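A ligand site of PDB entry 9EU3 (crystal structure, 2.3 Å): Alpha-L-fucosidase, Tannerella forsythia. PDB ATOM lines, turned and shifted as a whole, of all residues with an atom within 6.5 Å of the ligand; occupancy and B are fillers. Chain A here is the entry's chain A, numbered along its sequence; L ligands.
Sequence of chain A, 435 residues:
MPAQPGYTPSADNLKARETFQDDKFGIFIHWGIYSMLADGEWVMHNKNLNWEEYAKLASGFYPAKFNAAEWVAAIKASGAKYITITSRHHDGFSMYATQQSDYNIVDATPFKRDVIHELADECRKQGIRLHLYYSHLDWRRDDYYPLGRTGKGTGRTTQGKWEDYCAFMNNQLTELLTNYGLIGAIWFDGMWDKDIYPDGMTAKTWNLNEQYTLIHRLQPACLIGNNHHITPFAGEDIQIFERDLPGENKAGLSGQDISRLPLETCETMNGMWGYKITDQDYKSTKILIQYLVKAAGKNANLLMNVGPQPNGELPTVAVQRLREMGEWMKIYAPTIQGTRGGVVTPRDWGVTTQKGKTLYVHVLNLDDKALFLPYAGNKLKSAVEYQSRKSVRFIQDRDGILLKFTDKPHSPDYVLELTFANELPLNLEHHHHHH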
ATOM      1  N   PHE A  28      28.224   3.148  12.534  1.00  0.00           N
ATOM      2  CA  PHE A  28      27.110   2.217  12.633  1.00  0.00           C
ATOM      3  C   PHE A  28      26.609   2.187  14.072  1.00  0.00           C
ATOM      4  O   PHE A  28      27.416   2.235  15.010  1.00  0.00           O
ATOM      5  CB  PHE A  28      27.546   0.810  12.209  1.00  0.00           C
ATOM      6  CG  PHE A  28      26.560   0.072  11.339  1.00  0.00           C
ATOM      7  CD1 PHE A  28      25.206   0.349  11.384  1.00  0.00           C
ATOM      8  CD2 PHE A  28      27.015  -0.920  10.470  1.00  0.00           C
ATOM      9  CE1 PHE A  28      24.328  -0.344  10.583  1.00  0.00           C
ATOM     10  CE2 PHE A  28      26.141  -1.602   9.661  1.00  0.00           C
ATOM     11  CZ  PHE A  28      24.797  -1.321   9.715  1.00  0.00           C
ATOM     12  N   HIS A  30      23.916  -0.206  16.316  1.00  0.00           N
ATOM     13  CA  HIS A  30      22.996  -1.314  16.502  1.00  0.00           C
ATOM     14  C   HIS A  30      22.421  -1.201  17.911  1.00  0.00           C
ATOM     15  O   HIS A  30      23.107  -1.499  18.894  1.00  0.00           O
ATOM     16  CB  HIS A  30      23.698  -2.653  16.292  1.00  0.00           C
ATOM     17  CG  HIS A  30      23.853  -3.026  14.855  1.00  0.00           C
ATOM     18  ND1 HIS A  30      24.758  -2.394  14.024  1.00  0.00           N
ATOM     19  CD2 HIS A  30      23.214  -3.937  14.086  1.00  0.00           C
ATOM     20  CE1 HIS A  30      24.680  -2.913  12.819  1.00  0.00           C
ATOM     21  NE2 HIS A  30      23.753  -3.854  12.823  1.00  0.00           N
ATOM     22  N   GLU A  41      22.953  -8.928  19.068  1.00  0.00           N
ATOM     23  CA  GLU A  41      21.653  -8.650  18.482  1.00  0.00           C
ATOM     24  C   GLU A  41      20.950  -9.899  17.956  1.00  0.00           C
ATOM     25  O   GLU A  41      19.762  -9.823  17.635  1.00  0.00           O
ATOM     26  CB  GLU A  41      21.788  -7.637  17.343  1.00  0.00           C
ATOM     27  CG  GLU A  41      22.373  -8.195  16.052  1.00  0.00           C
ATOM     28  CD  GLU A  41      23.871  -8.436  16.116  1.00  0.00           C
ATOM     29  OE1 GLU A  41      24.471  -8.222  17.194  1.00  0.00           O
ATOM     30  OE2 GLU A  41      24.456  -8.837  15.090  1.00  0.00           O
ATOM     31  N   TRP A  42      21.641 -11.021  17.834  1.00  0.00           N
ATOM     32  CA  TRP A  42      21.053 -12.255  17.317  1.00  0.00           C
ATOM     33  C   TRP A  42      20.498 -13.153  18.415  1.00  0.00           C
ATOM     34  O   TRP A  42      20.159 -14.317  18.130  1.00  0.00           O
ATOM     35  CB  TRP A  42      22.086 -13.030  16.515  1.00  0.00           C
ATOM     36  CG  TRP A  42      22.115 -12.696  15.060  1.00  0.00           C
ATOM     37  CD1 TRP A  42      22.461 -11.505  14.491  1.00  0.00           C
ATOM     38  CD2 TRP A  42      21.803 -13.591  13.974  1.00  0.00           C
ATOM     39  NE1 TRP A  42      22.374 -11.591  13.119  1.00  0.00           N
ATOM     40  CE2 TRP A  42      21.974 -12.862  12.780  1.00  0.00           C
ATOM     41  CE3 TRP A  42      21.392 -14.916  13.902  1.00  0.00           C
ATOM     42  CZ2 TRP A  42      21.742 -13.424  11.524  1.00  0.00           C
ATOM     43  CZ3 TRP A  42      21.169 -15.474  12.655  1.00  0.00           C
ATOM     44  CH2 TRP A  42      21.341 -14.732  11.488  1.00  0.00           C
ATOM     45  N   THR A  86      20.059   1.356  13.341  1.00  0.00           N
ATOM     46  CA  THR A  86      19.038   0.319  13.149  1.00  0.00           C
ATOM     47  C   THR A  86      17.638   0.854  13.459  1.00  0.00           C
ATOM     48  O   THR A  86      17.304   1.104  14.618  1.00  0.00           O
ATOM     49  CB  THR A  86      19.336  -0.880  14.035  1.00  0.00           C
ATOM     50  OG1 THR A  86      19.500  -0.437  15.395  1.00  0.00           O
ATOM     51  CG2 THR A  86      20.606  -1.577  13.585  1.00  0.00           C
ATOM     52  N   HIS A  89      15.597  -4.299  13.483  1.00  0.00           N
ATOM     53  CA  HIS A  89      16.499  -5.397  13.215  1.00  0.00           C
ATOM     54  C   HIS A  89      15.727  -6.706  13.076  1.00  0.00           C
ATOM     55  O   HIS A  89      14.506  -6.715  12.904  1.00  0.00           O
ATOM     56  CB  HIS A  89      17.580  -5.483  14.296  1.00  0.00           C
ATOM     57  CG  HIS A  89      18.857  -6.087  13.800  1.00  0.00           C
ATOM     58  ND1 HIS A  89      19.163  -7.419  13.974  1.00  0.00           N
ATOM     59  CD2 HIS A  89      19.868  -5.561  13.082  1.00  0.00           C
ATOM     60  CE1 HIS A  89      20.326  -7.687  13.401  1.00  0.00           C
ATOM     61  NE2 HIS A  89      20.776  -6.570  12.857  1.00  0.00           N
ATOM     62  N   HIS A  90      16.448  -7.835  13.110  1.00  0.00           N
ATOM     63  CA  HIS A  90      15.811  -9.114  12.798  1.00  0.00           C
ATOM     64  C   HIS A  90      14.701  -9.456  13.782  1.00  0.00           C
ATOM     65  O   HIS A  90      13.781 -10.209  13.426  1.00  0.00           O
ATOM     66  CB  HIS A  90      16.838 -10.246  12.788  1.00  0.00           C
ATOM     67  CG  HIS A  90      18.004 -10.017  11.876  1.00  0.00           C
ATOM     68  ND1 HIS A  90      17.932  -9.195  10.761  1.00  0.00           N
ATOM     69  CD2 HIS A  90      19.263 -10.498  11.899  1.00  0.00           C
ATOM     70  CE1 HIS A  90      19.100  -9.174  10.163  1.00  0.00           C
ATOM     71  NE2 HIS A  90      19.930  -9.961  10.823  1.00  0.00           N
ATOM     72  N   TYR A 133      19.127   1.721   8.825  1.00  0.00           N
ATOM     73  CA  TYR A 133      19.161   0.277   8.601  1.00  0.00           C
ATOM     74  C   TYR A 133      17.765  -0.287   8.775  1.00  0.00           C
ATOM     75  O   TYR A 133      17.052   0.074   9.719  1.00  0.00           O
ATOM     76  CB  TYR A 133      20.154  -0.360   9.589  1.00  0.00           C
ATOM     77  CG  TYR A 133      20.136  -1.877   9.685  1.00  0.00           C
ATOM     78  CD1 TYR A 133      19.049  -2.545  10.227  1.00  0.00           C
ATOM     79  CD2 TYR A 133      21.214  -2.625   9.251  1.00  0.00           C
ATOM     80  CE1 TYR A 133      19.039  -3.930  10.314  1.00  0.00           C
ATOM     81  CE2 TYR A 133      21.211  -3.990   9.343  1.00  0.00           C
ATOM     82  CZ  TYR A 133      20.119  -4.637   9.872  1.00  0.00           C
ATOM     83  OH  TYR A 133      20.096  -6.011   9.969  1.00  0.00           O
ATOM     84  N   TRP A 187      19.498   1.119   4.251  1.00  0.00           N
ATOM     85  CA  TRP A 187      20.515   0.076   4.348  1.00  0.00           C
ATOM     86  C   TRP A 187      19.745  -1.208   4.626  1.00  0.00           C
ATOM     87  O   TRP A 187      19.486  -1.545   5.790  1.00  0.00           O
ATOM     88  CB  TRP A 187      21.470   0.418   5.471  1.00  0.00           C
ATOM     89  CG  TRP A 187      22.919   0.037   5.329  1.00  0.00           C
ATOM     90  CD1 TRP A 187      23.930   0.818   4.857  1.00  0.00           C
ATOM     91  CD2 TRP A 187      23.519  -1.198   5.739  1.00  0.00           C
ATOM     92  NE1 TRP A 187      25.128   0.143   4.941  1.00  0.00           N
ATOM     93  CE2 TRP A 187      24.901  -1.091   5.472  1.00  0.00           C
ATOM     94  CE3 TRP A 187      23.026  -2.386   6.294  1.00  0.00           C
ATOM     95  CZ2 TRP A 187      25.788  -2.140   5.738  1.00  0.00           C
ATOM     96  CZ3 TRP A 187      23.911  -3.418   6.556  1.00  0.00           C
ATOM     97  CH2 TRP A 187      25.277  -3.281   6.272  1.00  0.00           C
ATOM     98  N   ASP A 189      19.048  -5.193   4.923  1.00  0.00           N
ATOM     99  CA  ASP A 189      19.848  -6.331   5.334  1.00  0.00           C
ATOM    100  C   ASP A 189      18.909  -7.493   5.607  1.00  0.00           C
ATOM    101  O   ASP A 189      17.803  -7.292   6.133  1.00  0.00           O
ATOM    102  CB  ASP A 189      20.692  -6.011   6.568  1.00  0.00           C
ATOM    103  CG  ASP A 189      21.476  -7.207   7.075  1.00  0.00           C
ATOM    104  OD1 ASP A 189      21.972  -8.002   6.244  1.00  0.00           O
ATOM    105  OD2 ASP A 189      21.591  -7.352   8.313  1.00  0.00           O
ATOM    106  N   GLY A 190      19.336  -8.699   5.253  1.00  0.00           N
ATOM    107  CA  GLY A 190      18.662  -9.915   5.682  1.00  0.00           C
ATOM    108  C   GLY A 190      18.110 -10.814   4.591  1.00  0.00           C
ATOM    109  O   GLY A 190      17.644 -11.907   4.913  1.00  0.00           O
ATOM    110  N   TRP A 192      19.626 -12.563   2.509  1.00  0.00           N
ATOM    111  CA  TRP A 192      20.426 -13.782   2.514  1.00  0.00           C
ATOM    112  C   TRP A 192      19.777 -14.884   3.340  1.00  0.00           C
ATOM    113  O   TRP A 192      20.243 -16.028   3.280  1.00  0.00           O
ATOM    114  CB  TRP A 192      21.835 -13.496   3.076  1.00  0.00           C
ATOM    115  CG  TRP A 192      21.836 -12.539   4.231  1.00  0.00           C
ATOM    116  CD1 TRP A 192      22.259 -11.250   4.217  1.00  0.00           C
ATOM    117  CD2 TRP A 192      21.389 -12.812   5.567  1.00  0.00           C
ATOM    118  NE1 TRP A 192      22.098 -10.683   5.459  1.00  0.00           N
ATOM    119  CE2 TRP A 192      21.572 -11.626   6.314  1.00  0.00           C
ATOM    120  CE3 TRP A 192      20.859 -13.938   6.205  1.00  0.00           C
ATOM    121  CZ2 TRP A 192      21.233 -11.531   7.665  1.00  0.00           C
ATOM    122  CZ3 TRP A 192      20.523 -13.845   7.542  1.00  0.00           C
ATOM    123  CH2 TRP A 192      20.709 -12.648   8.258  1.00  0.00           C
ATOM    124  N   ASN A 227      22.686  -5.354   1.918  1.00  0.00           N
ATOM    125  CA  ASN A 227      23.760  -6.242   2.360  1.00  0.00           C
ATOM    126  C   ASN A 227      23.433  -7.695   2.015  1.00  0.00           C
ATOM    127  O   ASN A 227      23.241  -8.544   2.887  1.00  0.00           O
ATOM    128  CB  ASN A 227      23.997  -6.070   3.848  1.00  0.00           C
ATOM    129  CG  ASN A 227      25.153  -6.900   4.351  1.00  0.00           C
ATOM    130  OD1 ASN A 227      26.099  -7.189   3.611  1.00  0.00           O
ATOM    131  ND2 ASN A 227      25.105  -7.292   5.620  1.00  0.00           N
ATOM    132  N   HIS A 229      25.505  -9.464  -0.108  1.00  0.00           N
ATOM    133  CA  HIS A 229      26.792 -10.099  -0.381  1.00  0.00           C
ATOM    134  C   HIS A 229      26.932 -10.584  -1.822  1.00  0.00           C
ATOM    135  O   HIS A 229      27.794 -11.420  -2.121  1.00  0.00           O
ATOM    136  CB  HIS A 229      27.058 -11.256   0.578  1.00  0.00           C
ATOM    137  CG  HIS A 229      26.986 -10.881   2.020  1.00  0.00           C
ATOM    138  ND1 HIS A 229      26.618 -11.774   3.006  1.00  0.00           N
ATOM    139  CD2 HIS A 229      27.182  -9.702   2.646  1.00  0.00           C
ATOM    140  CE1 HIS A 229      26.633 -11.164   4.179  1.00  0.00           C
ATOM    141  NE2 HIS A 229      26.961  -9.902   3.985  1.00  0.00           N
ATOM    142  N   GLU A 242      30.716  -6.661   4.065  1.00  0.00           N
ATOM    143  CA  GLU A 242      30.564  -6.890   5.493  1.00  0.00           C
ATOM    144  C   GLU A 242      31.878  -7.430   6.051  1.00  0.00           C
ATOM    145  O   GLU A 242      32.286  -8.535   5.711  1.00  0.00           O
ATOM    146  CB  GLU A 242      29.400  -7.848   5.769  1.00  0.00           C
ATOM    147  CG  GLU A 242      29.109  -8.055   7.256  1.00  0.00           C
ATOM    148  CD  GLU A 242      27.900  -8.956   7.526  1.00  0.00           C
ATOM    149  OE1 GLU A 242      27.803  -9.503   8.651  1.00  0.00           O
ATOM    150  OE2 GLU A 242      27.056  -9.121   6.624  1.00  0.00           O
ATOM    151  N   ARG A 243      32.526  -6.642   6.905  1.00  0.00           N
ATOM    152  CA  ARG A 243      33.717  -7.071   7.642  1.00  0.00           C
ATOM    153  C   ARG A 243      34.895  -7.395   6.714  1.00  0.00           C
ATOM    154  O   ARG A 243      35.719  -8.260   7.018  1.00  0.00           O
ATOM    155  CB  ARG A 243      33.417  -8.290   8.523  1.00  0.00           C
ATOM    156  CG  ARG A 243      32.379  -8.078   9.595  1.00  0.00           C
ATOM    157  CD  ARG A 243      32.155  -9.380  10.347  1.00  0.00           C
ATOM    158  NE  ARG A 243      31.317  -9.241  11.533  1.00  0.00           N
ATOM    159  CZ  ARG A 243      31.762  -8.882  12.723  1.00  0.00           C
ATOM    160  NH1 ARG A 243      33.008  -8.493  12.909  1.00  0.00           N
ATOM    161  NH2 ARG A 243      30.918  -8.898  13.760  1.00  0.00           N
ATOM    162  N   LEU A 253      32.407 -13.501   4.411  1.00  0.00           N
ATOM    163  CA  LEU A 253      31.078 -13.011   4.088  1.00  0.00           C
ATOM    164  C   LEU A 253      31.038 -12.213   2.793  1.00  0.00           C
ATOM    165  O   LEU A 253      30.051 -11.499   2.546  1.00  0.00           O
ATOM    166  CB  LEU A 253      30.541 -12.159   5.238  1.00  0.00           C
ATOM    167  CG  LEU A 253      30.705 -12.666   6.669  1.00  0.00           C
ATOM    168  CD1 LEU A 253      30.234 -11.594   7.666  1.00  0.00           C
ATOM    169  CD2 LEU A 253      29.938 -13.963   6.862  1.00  0.00           C
ATOM    170  N   CYS A 266      31.648  -2.328   6.175  1.00  0.00           N
ATOM    171  CA  CYS A 266      31.177  -2.189   7.545  1.00  0.00           C
ATOM    172  C   CYS A 266      31.952  -3.127   8.472  1.00  0.00           C
ATOM    173  O   CYS A 266      32.292  -4.248   8.082  1.00  0.00           O
ATOM    174  CB  CYS A 266      29.672  -2.464   7.667  1.00  0.00           C
ATOM    175  SG  CYS A 266      29.115  -4.106   7.207  1.00  0.00           S
ATOM    176  N   TRP A 273      28.045  -6.459  16.798  1.00  0.00           N
ATOM    177  CA  TRP A 273      27.293  -5.271  16.412  1.00  0.00           C
ATOM    178  C   TRP A 273      26.473  -4.747  17.594  1.00  0.00           C
ATOM    179  O   TRP A 273      26.638  -3.586  18.009  1.00  0.00           O
ATOM    180  CB  TRP A 273      26.399  -5.600  15.226  1.00  0.00           C
ATOM    181  CG  TRP A 273      27.124  -6.243  14.066  1.00  0.00           C
ATOM    182  CD1 TRP A 273      27.166  -7.580  13.757  1.00  0.00           C
ATOM    183  CD2 TRP A 273      27.910  -5.573  13.067  1.00  0.00           C
ATOM    184  NE1 TRP A 273      27.922  -7.780  12.622  1.00  0.00           N
ATOM    185  CE2 TRP A 273      28.382  -6.566  12.180  1.00  0.00           C
ATOM    186  CE3 TRP A 273      28.242  -4.243  12.831  1.00  0.00           C
ATOM    187  CZ2 TRP A 273      29.187  -6.259  11.078  1.00  0.00           C
ATOM    188  CZ3 TRP A 273      29.034  -3.937  11.733  1.00  0.00           C
ATOM    189  CH2 TRP A 273      29.498  -4.937  10.868  1.00  0.00           C
HETATM  190  C1  LIG L   1      24.751  -8.802   9.251  1.00  0.00           C
HETATM  191  C2  LIG L   1      23.617  -8.829  10.265  1.00  0.00           C
HETATM  192  O1  LIG L   1      23.168 -10.172  10.528  1.00  0.00           O
HETATM  193  C3  LIG L   1      24.087  -8.233  11.550  1.00  0.00           C
HETATM  194  O2  LIG L   1      23.062  -8.366  12.573  1.00  0.00           O
HETATM  195  C4  LIG L   1      24.443  -6.792  11.438  1.00  0.00           C
HETATM  196  O3  LIG L   1      23.262  -6.008  11.346  1.00  0.00           O
HETATM  197  C5  LIG L   1      25.304  -6.519  10.201  1.00  0.00           C
HETATM  198  C6  LIG L   1      24.491  -5.778   9.176  1.00  0.00           C
HETATM  199  O4  LIG L   1      25.793  -7.747   9.556  1.00  0.00           O
HETATM  200  O5  LIG L   1      24.206  -8.561   8.025  1.00  0.00           O
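A ring nitrogen (NE2) of His 30 is in hydrogen-bond range of an oxygen (O3) of the ligand, 2.7 Å away. An oxygen (O5) of the ligand sits at hydrogen-bond distance from the side-chain carboxylate (OE2) of Glu 242, 3.2 Å away. ND2 of Asn 227 sits at hydrogen-bond distance from O5 of the ligand, 2.9 Å away. OD2 of Asp 189 sits at hydrogen-bond distance from O5 of the ligand, 2.9 Å away. An oxygen (O2) of the ligand sits at hydrogen-bond distance from the side-chain carboxylate (OE2) of Glu 41 (2.9 Å). A ring nitrogen (NE2) of His 89 sits at hydrogen-bond distance from an oxygen (O2) of the ligand, at 2.9 Å. O1 of the ligand lies within hydrogen-bond range of NE1 of Trp 42, at 3.1 Å. A ring nitrogen (NE2) of His 90 sits at hydrogen-bond distance from an oxygen (O1) of the ligand, 3.3 Å away. OH of Tyr 133 lies within hydrogen-bond range of O3 of the ligand (3.5 Å).
OE2 of Glu 242 lies within hydrogen-bond range of ND2 of Asn 227. OE2 of Glu 242 sits at hydrogen-bond distance from NE2 of His 229 (2.8 Å). The side-chain amide nitrogen (ND2) of Asn 227 sits at hydrogen-bond distance from the side-chain carboxylate (OD1) of Asp 189, 3.3 Å away. The side-chain amide oxygen of Asn 227 lies within hydrogen-bond range of a ring nitrogen (NE2) of His 229, at 2.9 Å. The side-chain hydroxyl (OH) of Tyr 133 sits at hydrogen-bond distance from the side-chain carboxylate (OD2) of Asp 189, 2.6 Å away. The side-chain carboxylate of Asp 189 sits at hydrogen-bond distance from the indole nitrogen of Trp 192 (2.8 Å). A ring nitrogen (NE2) of His 89 sits at hydrogen-bond distance from the side-chain hydroxyl (OH) of Tyr 133 (3.0 Å).
Residues that only touch the ligand: Trp 187, Trp 273 and Trp 192. Hydrophobic or aromatic side chains that line the ligand: His 30, Trp 42, His 89, Tyr 133, Trp 187, Trp 192 and Trp 273. Of the 19 residues printed, 12 come within 4 Å of the ligand.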
